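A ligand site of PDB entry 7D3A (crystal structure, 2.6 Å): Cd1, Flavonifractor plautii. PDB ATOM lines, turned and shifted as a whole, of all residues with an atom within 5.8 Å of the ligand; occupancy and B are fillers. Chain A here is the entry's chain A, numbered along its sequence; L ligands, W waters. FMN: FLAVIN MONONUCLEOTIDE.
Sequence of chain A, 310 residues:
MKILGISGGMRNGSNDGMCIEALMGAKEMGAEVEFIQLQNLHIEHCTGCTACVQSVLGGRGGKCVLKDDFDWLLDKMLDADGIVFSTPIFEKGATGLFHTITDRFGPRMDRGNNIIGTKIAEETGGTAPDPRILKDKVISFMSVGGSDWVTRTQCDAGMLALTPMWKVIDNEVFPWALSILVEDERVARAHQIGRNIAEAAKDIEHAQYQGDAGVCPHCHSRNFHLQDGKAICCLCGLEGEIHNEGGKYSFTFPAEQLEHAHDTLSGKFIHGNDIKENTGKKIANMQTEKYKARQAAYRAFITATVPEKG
The backbone NH (N) of Ser 147 sits at hydrogen-bond distance from an oxygen (O2) of the ligand (2.7 Å). An oxygen (O2) of the ligand sits close to the backbone carbonyl oxygen (O) of Ser 147, at 2.7 Å. OG of Ser 147 lies close to O2 of the ligand (3.4 Å). The backbone NH (N) of Gly 146 lies within hydrogen-bond range of an oxygen (O2) of the ligand. The backbone carbonyl oxygen of Trp 149 is in hydrogen-bond range of a nitrogen (N3) of the ligand (2.7 Å). An oxygen (O4') of the ligand lies within hydrogen-bond range of the backbone carbonyl oxygen (O) of Val 144 (2.7 Å). The backbone NH (N) of Ile 89 is in hydrogen-bond range of an oxygen (O2') of the ligand. O of Ile 89 lies within hydrogen-bond range of O2' of the ligand (2.7 Å). N of Ser 14 sits at hydrogen-bond distance from O3P of the ligand (2.8 Å). The side-chain hydroxyl (OG) of Ser 14 lies within hydrogen-bond range of an oxygen (O3P) of the ligand (3.4 Å). The backbone NH (N) of Lys 92 is in hydrogen-bond range of an oxygen (O4) of the ligand (2.9 Å). N of Met 10 sits at hydrogen-bond distance from O2P of the ligand (2.9 Å). N of Asn 15 sits at hydrogen-bond distance from O1P of the ligand (3.0 Å). The side-chain amide nitrogen (ND2) of Asn 15 lies within hydrogen-bond range of an oxygen (O1P) of the ligand (3.0 Å). The backbone NH (N) of Glu 91 lies within hydrogen-bond range of a nitrogen (N5) of the ligand (3.0 Å).
OG of Ser 147 sits at hydrogen-bond distance from N of Trp 149, 3.0 Å away. The backbone carbonyl oxygen (O) of Val 144 is in hydrogen-bond range of the backbone NH (N) of Ile 89, at 3.1 Å. The backbone carbonyl oxygen (O) of Thr 87 sits at hydrogen-bond distance from the backbone NH (N) of Val 144. O of Thr 87 lies close to OD1 of Asn 15. The backbone NH of Gly 9 lies within hydrogen-bond range of the side-chain hydroxyl of Ser 7 (3.2 Å).
Merely in contact with the ligand: Gly 145, Gly 9, Phe 90, Gly 13 and Pro 88. Hydrophobic or aromatic side chains within 4 Å of the ligand: Met 10, Pro 88, Ile 89, Phe 90 and Trp 149. Of the 25 residues printed, 15 come within 4 Å of the ligand.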
ATOM      1  N   SER A   7     -10.918   5.439  16.273  1.00  0.00           N
ATOM      2  CA  SER A   7      -9.633   5.044  15.709  1.00  0.00           C
ATOM      3  C   SER A   7      -9.803   3.873  14.751  1.00  0.00           C
ATOM      4  O   SER A   7     -10.518   2.919  15.045  1.00  0.00           O
ATOM      5  CB  SER A   7      -8.629   4.655  16.784  1.00  0.00           C
ATOM      6  OG  SER A   7      -7.519   4.007  16.169  1.00  0.00           O
ATOM      7  N   GLY A   8      -9.102   3.957  13.614  1.00  0.00           N
ATOM      8  CA  GLY A   8      -9.108   2.904  12.621  1.00  0.00           C
ATOM      9  C   GLY A   8      -7.830   2.087  12.597  1.00  0.00           C
ATOM     10  O   GLY A   8      -7.671   1.223  11.730  1.00  0.00           O
ATOM     11  N   GLY A   9      -6.906   2.326  13.526  1.00  0.00           N
ATOM     12  CA  GLY A   9      -5.657   1.604  13.538  1.00  0.00           C
ATOM     13  C   GLY A   9      -5.773   0.288  14.286  1.00  0.00           C
ATOM     14  O   GLY A   9      -6.864  -0.175  14.636  1.00  0.00           O
ATOM     15  N   MET A  10      -4.607  -0.350  14.508  1.00  0.00           N
ATOM     16  CA  MET A  10      -4.534  -1.554  15.376  1.00  0.00           C
ATOM     17  C   MET A  10      -4.767  -1.138  16.823  1.00  0.00           C
ATOM     18  O   MET A  10      -4.431  -0.012  17.226  1.00  0.00           O
ATOM     19  CB  MET A  10      -3.178  -2.283  15.264  1.00  0.00           C
ATOM     20  CG  MET A  10      -2.957  -3.173  14.003  1.00  0.00           C
ATOM     21  SD  MET A  10      -4.311  -4.561  13.501  1.00  0.00           S
ATOM     22  CE  MET A  10      -4.919  -5.137  15.281  1.00  0.00           C
ATOM     23  N   GLY A  13      -2.370   1.138  18.922  1.00  0.00           N
ATOM     24  CA  GLY A  13      -1.433   1.702  17.981  1.00  0.00           C
ATOM     25  C   GLY A  13      -1.393   3.214  18.003  1.00  0.00           C
ATOM     26  O   GLY A  13      -1.971   3.875  18.883  1.00  0.00           O
ATOM     27  N   SER A  14      -0.736   3.779  16.989  1.00  0.00           N
ATOM     28  CA  SER A  14      -0.518   5.218  16.960  1.00  0.00           C
ATOM     29  C   SER A  14      -1.827   5.978  16.749  1.00  0.00           C
ATOM     30  O   SER A  14      -2.043   7.045  17.353  1.00  0.00           O
ATOM     31  CB  SER A  14       0.515   5.558  15.892  1.00  0.00           C
ATOM     32  OG  SER A  14       1.595   4.615  15.910  1.00  0.00           O
ATOM     33  N   ASN A  15      -2.722   5.459  15.902  1.00  0.00           N
ATOM     34  CA  ASN A  15      -3.991   6.135  15.713  1.00  0.00           C
ATOM     35  C   ASN A  15      -4.809   6.169  17.003  1.00  0.00           C
ATOM     36  O   ASN A  15      -5.419   7.193  17.319  1.00  0.00           O
ATOM     37  CB  ASN A  15      -4.768   5.489  14.564  1.00  0.00           C
ATOM     38  CG  ASN A  15      -4.242   5.913  13.191  1.00  0.00           C
ATOM     39  OD1 ASN A  15      -4.638   6.954  12.651  1.00  0.00           O
ATOM     40  ND2 ASN A  15      -3.359   5.104  12.610  1.00  0.00           N
ATOM     41  N   ASP A  16      -4.807   5.073  17.764  1.00  0.00           N
ATOM     42  CA  ASP A  16      -5.360   5.072  19.134  1.00  0.00           C
ATOM     43  C   ASP A  16      -4.796   6.216  19.969  1.00  0.00           C
ATOM     44  O   ASP A  16      -5.553   7.012  20.546  1.00  0.00           O
ATOM     45  CB  ASP A  16      -5.059   3.744  19.831  1.00  0.00           C
ATOM     46  CG  ASP A  16      -5.987   2.582  19.416  1.00  0.00           C
ATOM     47  OD1 ASP A  16      -6.732   2.730  18.425  1.00  0.00           O
ATOM     48  OD2 ASP A  16      -5.944   1.515  20.065  1.00  0.00           O
ATOM     49  N   THR A  87      -7.667   7.794  11.176  1.00  0.00           N
ATOM     50  CA  THR A  87      -7.458   6.624  10.351  1.00  0.00           C
ATOM     51  C   THR A  87      -6.006   6.439   9.936  1.00  0.00           C
ATOM     52  O   THR A  87      -5.321   7.386   9.726  1.00  0.00           O
ATOM     53  CB  THR A  87      -8.392   6.619   9.112  1.00  0.00           C
ATOM     54  OG1 THR A  87      -8.283   5.396   8.390  1.00  0.00           O
ATOM     55  CG2 THR A  87      -8.093   7.750   8.205  1.00  0.00           C
ATOM     56  N   PRO A  88      -5.574   5.203   9.796  1.00  0.00           N
ATOM     57  CA  PRO A  88      -4.311   4.926   9.105  1.00  0.00           C
ATOM     58  C   PRO A  88      -4.415   5.235   7.619  1.00  0.00           C
ATOM     59  O   PRO A  88      -5.493   5.289   7.033  1.00  0.00           O
ATOM     60  CB  PRO A  88      -4.106   3.415   9.323  1.00  0.00           C
ATOM     61  CG  PRO A  88      -5.171   2.997  10.326  1.00  0.00           C
ATOM     62  CD  PRO A  88      -6.287   3.963  10.144  1.00  0.00           C
ATOM     63  N   ILE A  89      -3.271   5.433   6.999  1.00  0.00           N
ATOM     64  CA  ILE A  89      -3.202   5.636   5.566  1.00  0.00           C
ATOM     65  C   ILE A  89      -2.822   4.318   4.915  1.00  0.00           C
ATOM     66  O   ILE A  89      -1.818   3.707   5.281  1.00  0.00           O
ATOM     67  CB  ILE A  89      -2.210   6.753   5.233  1.00  0.00           C
ATOM     68  CG1 ILE A  89      -2.712   8.075   5.831  1.00  0.00           C
ATOM     69  CG2 ILE A  89      -2.031   6.898   3.726  1.00  0.00           C
ATOM     70  CD1 ILE A  89      -1.725   9.211   5.731  1.00  0.00           C
ATOM     71  N   PHE A  90      -3.660   3.852   3.993  1.00  0.00           N
ATOM     72  CA  PHE A  90      -3.405   2.672   3.169  1.00  0.00           C
ATOM     73  C   PHE A  90      -3.413   3.134   1.716  1.00  0.00           C
ATOM     74  O   PHE A  90      -4.359   3.789   1.275  1.00  0.00           O
ATOM     75  CB  PHE A  90      -4.452   1.564   3.359  1.00  0.00           C
ATOM     76  CG  PHE A  90      -4.395   0.857   4.706  1.00  0.00           C
ATOM     77  CD1 PHE A  90      -5.226  -0.225   4.967  1.00  0.00           C
ATOM     78  CD2 PHE A  90      -3.530   1.287   5.706  1.00  0.00           C
ATOM     79  CE1 PHE A  90      -5.189  -0.885   6.200  1.00  0.00           C
ATOM     80  CE2 PHE A  90      -3.475   0.641   6.933  1.00  0.00           C
ATOM     81  CZ  PHE A  90      -4.310  -0.451   7.187  1.00  0.00           C
ATOM     82  N   GLU A  91      -2.345   2.795   0.982  1.00  0.00           N
ATOM     83  CA  GLU A  91      -2.133   3.202  -0.415  1.00  0.00           C
ATOM     84  C   GLU A  91      -2.519   4.654  -0.675  1.00  0.00           C
ATOM     85  O   GLU A  91      -3.217   4.955  -1.657  1.00  0.00           O
ATOM     86  CB  GLU A  91      -2.876   2.307  -1.381  1.00  0.00           C
ATOM     87  CG  GLU A  91      -2.545   0.864  -1.264  1.00  0.00           C
ATOM     88  CD  GLU A  91      -3.503   0.162  -0.331  1.00  0.00           C
ATOM     89  OE1 GLU A  91      -3.046  -0.580   0.547  1.00  0.00           O
ATOM     90  OE2 GLU A  91      -4.716   0.370  -0.481  1.00  0.00           O
ATOM     91  N   LYS A  92      -2.053   5.582   0.155  1.00  0.00           N
ATOM     92  CA  LYS A  92      -2.201   7.024  -0.021  1.00  0.00           C
ATOM     93  C   LYS A  92      -3.682   7.357   0.106  1.00  0.00           C
ATOM     94  O   LYS A  92      -4.205   8.095  -0.725  1.00  0.00           O
ATOM     95  CB  LYS A  92      -2.009   7.468  -1.489  1.00  0.00           C
ATOM     96  CG  LYS A  92      -0.822   6.807  -2.172  1.00  0.00           C
ATOM     97  CD  LYS A  92      -0.549   7.432  -3.545  1.00  0.00           C
ATOM     98  CE  LYS A  92       0.604   6.722  -4.215  1.00  0.00           C
ATOM     99  NZ  LYS A  92       1.041   7.465  -5.404  1.00  0.00           N
ATOM    100  N   GLY A  93      -4.377   6.835   1.119  1.00  0.00           N
ATOM    101  CA  GLY A  93      -5.784   7.184   1.297  1.00  0.00           C
ATOM    102  C   GLY A  93      -6.176   6.523   2.594  1.00  0.00           C
ATOM    103  O   GLY A  93      -5.322   5.949   3.295  1.00  0.00           O
ATOM    104  N   VAL A 144      -2.821   9.219   9.666  1.00  0.00           N
ATOM    105  CA  VAL A 144      -1.486   8.862  10.157  1.00  0.00           C
ATOM    106  C   VAL A 144      -0.905   7.794   9.232  1.00  0.00           C
ATOM    107  O   VAL A 144      -1.426   6.668   9.177  1.00  0.00           O
ATOM    108  CB  VAL A 144      -1.529   8.369  11.609  1.00  0.00           C
ATOM    109  CG1 VAL A 144      -0.104   8.124  12.133  1.00  0.00           C
ATOM    110  CG2 VAL A 144      -2.264   9.353  12.472  1.00  0.00           C
ATOM    111  N   GLY A 145       0.177   8.122   8.533  1.00  0.00           N
ATOM    112  CA  GLY A 145       0.823   7.221   7.611  1.00  0.00           C
ATOM    113  C   GLY A 145       2.258   6.948   8.036  1.00  0.00           C
ATOM    114  O   GLY A 145       2.812   7.629   8.902  1.00  0.00           O
ATOM    115  N   GLY A 146       2.847   5.932   7.423  1.00  0.00           N
ATOM    116  CA  GLY A 146       4.224   5.544   7.731  1.00  0.00           C
ATOM    117  C   GLY A 146       5.278   6.164   6.822  1.00  0.00           C
ATOM    118  O   GLY A 146       6.463   6.155   7.150  1.00  0.00           O
ATOM    119  N   SER A 147       4.853   6.699   5.682  1.00  0.00           N
ATOM    120  CA  SER A 147       5.775   7.392   4.784  1.00  0.00           C
ATOM    121  C   SER A 147       4.955   8.526   4.202  1.00  0.00           C
ATOM    122  O   SER A 147       3.792   8.723   4.585  1.00  0.00           O
ATOM    123  CB  SER A 147       6.081   6.541   3.547  1.00  0.00           C
ATOM    124  OG  SER A 147       4.948   6.451   2.711  1.00  0.00           O
ATOM    125  N   ASP A 148       5.555   9.272   3.273  1.00  0.00           N
ATOM    126  CA  ASP A 148       4.840  10.286   2.510  1.00  0.00           C
ATOM    127  C   ASP A 148       3.929   9.927   1.332  1.00  0.00           C
ATOM    128  O   ASP A 148       3.663  10.782   0.490  1.00  0.00           O
ATOM    129  CB  ASP A 148       5.902  11.295   2.065  1.00  0.00           C
ATOM    130  CG  ASP A 148       6.794  10.755   0.984  1.00  0.00           C
ATOM    131  OD1 ASP A 148       6.860   9.511   0.826  1.00  0.00           O
ATOM    132  OD2 ASP A 148       7.452  11.564   0.305  1.00  0.00           O
ATOM    133  N   TRP A 149       3.503   8.668   1.229  1.00  0.00           N
ATOM    134  CA  TRP A 149       2.452   8.289   0.280  1.00  0.00           C
ATOM    135  C   TRP A 149       1.118   8.632   0.927  1.00  0.00           C
ATOM    136  O   TRP A 149       0.441   7.788   1.520  1.00  0.00           O
ATOM    137  CB  TRP A 149       2.511   6.798  -0.044  1.00  0.00           C
ATOM    138  CG  TRP A 149       3.713   6.314  -0.789  1.00  0.00           C
ATOM    139  CD1 TRP A 149       4.971   6.853  -0.786  1.00  0.00           C
ATOM    140  CD2 TRP A 149       3.758   5.170  -1.647  1.00  0.00           C
ATOM    141  NE1 TRP A 149       5.805   6.105  -1.609  1.00  0.00           N
ATOM    142  CE2 TRP A 149       5.071   5.067  -2.144  1.00  0.00           C
ATOM    143  CE3 TRP A 149       2.811   4.228  -2.061  1.00  0.00           C
ATOM    144  CZ2 TRP A 149       5.457   4.058  -3.012  1.00  0.00           C
ATOM    145  CZ3 TRP A 149       3.201   3.231  -2.935  1.00  0.00           C
ATOM    146  CH2 TRP A 149       4.507   3.157  -3.404  1.00  0.00           C
ATOM    147  N   VAL A 150       0.735   9.910   0.835  1.00  0.00           N
ATOM    148  CA  VAL A 150      -0.388  10.391   1.646  1.00  0.00           C
ATOM    149  C   VAL A 150      -1.272  11.347   0.856  1.00  0.00           C
ATOM    150  O   VAL A 150      -2.061  12.095   1.432  1.00  0.00           O
ATOM    151  CB  VAL A 150       0.114  11.080   2.927  1.00  0.00           C
ATOM    152  CG1 VAL A 150       0.999  10.145   3.739  1.00  0.00           C
ATOM    153  CG2 VAL A 150       0.865  12.308   2.588  1.00  0.00           C
ATOM    154  N   PRO A 175       2.499  12.363   7.903  1.00  0.00           N
ATOM    155  CA  PRO A 175       3.387  11.411   7.236  1.00  0.00           C
ATOM    156  C   PRO A 175       4.531  11.003   8.146  1.00  0.00           C
ATOM    157  O   PRO A 175       4.781  11.627   9.178  1.00  0.00           O
ATOM    158  CB  PRO A 175       3.905  12.213   6.029  1.00  0.00           C
ATOM    159  CG  PRO A 175       3.865  13.625   6.501  1.00  0.00           C
ATOM    160  CD  PRO A 175       2.686  13.745   7.420  1.00  0.00           C
ATOM    161  N   TRP A 176       5.246   9.941   7.741  1.00  0.00           N
ATOM    162  CA  TRP A 176       6.419   9.488   8.481  1.00  0.00           C
ATOM    163  C   TRP A 176       6.104   9.375   9.970  1.00  0.00           C
ATOM    164  O   TRP A 176       6.791   9.951  10.818  1.00  0.00           O
ATOM    165  CB  TRP A 176       7.607  10.422   8.266  1.00  0.00           C
ATOM    166  CG  TRP A 176       7.910  10.747   6.842  1.00  0.00           C
ATOM    167  CD1 TRP A 176       7.701  11.941   6.210  1.00  0.00           C
ATOM    168  CD2 TRP A 176       8.467   9.867   5.847  1.00  0.00           C
ATOM    169  NE1 TRP A 176       8.094  11.866   4.892  1.00  0.00           N
ATOM    170  CE2 TRP A 176       8.578  10.611   4.640  1.00  0.00           C
ATOM    171  CE3 TRP A 176       8.886   8.536   5.862  1.00  0.00           C
ATOM    172  CZ2 TRP A 176       9.091  10.060   3.470  1.00  0.00           C
ATOM    173  CZ3 TRP A 176       9.386   7.982   4.677  1.00  0.00           C
ATOM    174  CH2 TRP A 176       9.485   8.743   3.505  1.00  0.00           C
ATOM    175  N   LEU A 178       5.351   6.413  11.871  1.00  0.00           N
ATOM    176  CA  LEU A 178       5.471   5.148  12.599  1.00  0.00           C
ATOM    177  C   LEU A 178       5.873   5.375  14.050  1.00  0.00           C
ATOM    178  O   LEU A 178       5.437   4.643  14.935  1.00  0.00           O
ATOM    179  CB  LEU A 178       6.470   4.220  11.907  1.00  0.00           C
ATOM    180  CG  LEU A 178       5.998   3.599  10.585  1.00  0.00           C
ATOM    181  CD1 LEU A 178       7.040   2.619  10.028  1.00  0.00           C
ATOM    182  CD2 LEU A 178       4.682   2.893  10.791  1.00  0.00           C
HETATM  183  N1  FMN L   1       1.614   4.544   5.015  1.00  0.00           N
HETATM  184  C2  FMN L   1       1.756   5.611   4.237  1.00  0.00           C
HETATM  185  O2  FMN L   1       2.319   6.529   4.843  1.00  0.00           O
HETATM  186  N3  FMN L   1       1.338   5.636   2.943  1.00  0.00           N
HETATM  187  C4  FMN L   1       0.715   4.550   2.440  1.00  0.00           C
HETATM  188  O4  FMN L   1       0.296   4.421   1.300  1.00  0.00           O
HETATM  189  C4A FMN L   1       0.554   3.357   3.286  1.00  0.00           C
HETATM  190  N5  FMN L   1      -0.019   2.261   2.862  1.00  0.00           N
HETATM  191  C5A FMN L   1      -0.216   1.183   3.624  1.00  0.00           C
HETATM  192  C6  FMN L   1      -0.851   0.044   3.155  1.00  0.00           C
HETATM  193  C7  FMN L   1      -1.034  -1.073   3.966  1.00  0.00           C
HETATM  194  C7M FMN L   1      -1.703  -2.311   3.438  1.00  0.00           C
HETATM  195  C8  FMN L   1      -0.531  -1.038   5.362  1.00  0.00           C
HETATM  196  C8M FMN L   1      -0.711  -2.246   6.243  1.00  0.00           C
HETATM  197  C9  FMN L   1       0.102   0.111   5.817  1.00  0.00           C
HETATM  198  C9A FMN L   1       0.260   1.211   5.005  1.00  0.00           C
HETATM  199  N10 FMN L   1       0.922   2.357   5.475  1.00  0.00           N
HETATM  200  C10 FMN L   1       1.044   3.429   4.633  1.00  0.00           C
HETATM  201  C1' FMN L   1       1.361   2.387   6.862  1.00  0.00           C
HETATM  202  C2' FMN L   1       0.194   2.684   7.804  1.00  0.00           C
HETATM  203  O2' FMN L   1      -0.369   3.974   7.600  1.00  0.00           O
HETATM  204  C3' FMN L   1       0.626   2.467   9.287  1.00  0.00           C
HETATM  205  O3' FMN L   1       0.978   1.141   9.526  1.00  0.00           O
HETATM  206  C4' FMN L   1      -0.444   2.969  10.291  1.00  0.00           C
HETATM  207  O4' FMN L   1      -0.499   4.379  10.366  1.00  0.00           O
HETATM  208  C5' FMN L   1      -0.215   2.340  11.658  1.00  0.00           C
HETATM  209  O5' FMN L   1      -1.137   2.772  12.609  1.00  0.00           O
HETATM  210  P   FMN L   1      -1.634   2.098  13.868  1.00  0.00           P
HETATM  211  O1P FMN L   1      -2.664   2.856  14.401  1.00  0.00           O
HETATM  212  O2P FMN L   1      -2.115   0.838  13.473  1.00  0.00           O
HETATM  213  O3P FMN L   1      -0.473   2.154  14.697  1.00  0.00           O
HETATM  214  O   HOH W   1      -1.000  -0.291   9.564  1.00  0.00           O
HETATM  215  O   HOH W   2      -3.061   0.322  11.125  1.00  0.00           O
HETATM  216  O   HOH W   3      -4.217   2.564  16.620  1.00  0.00           O
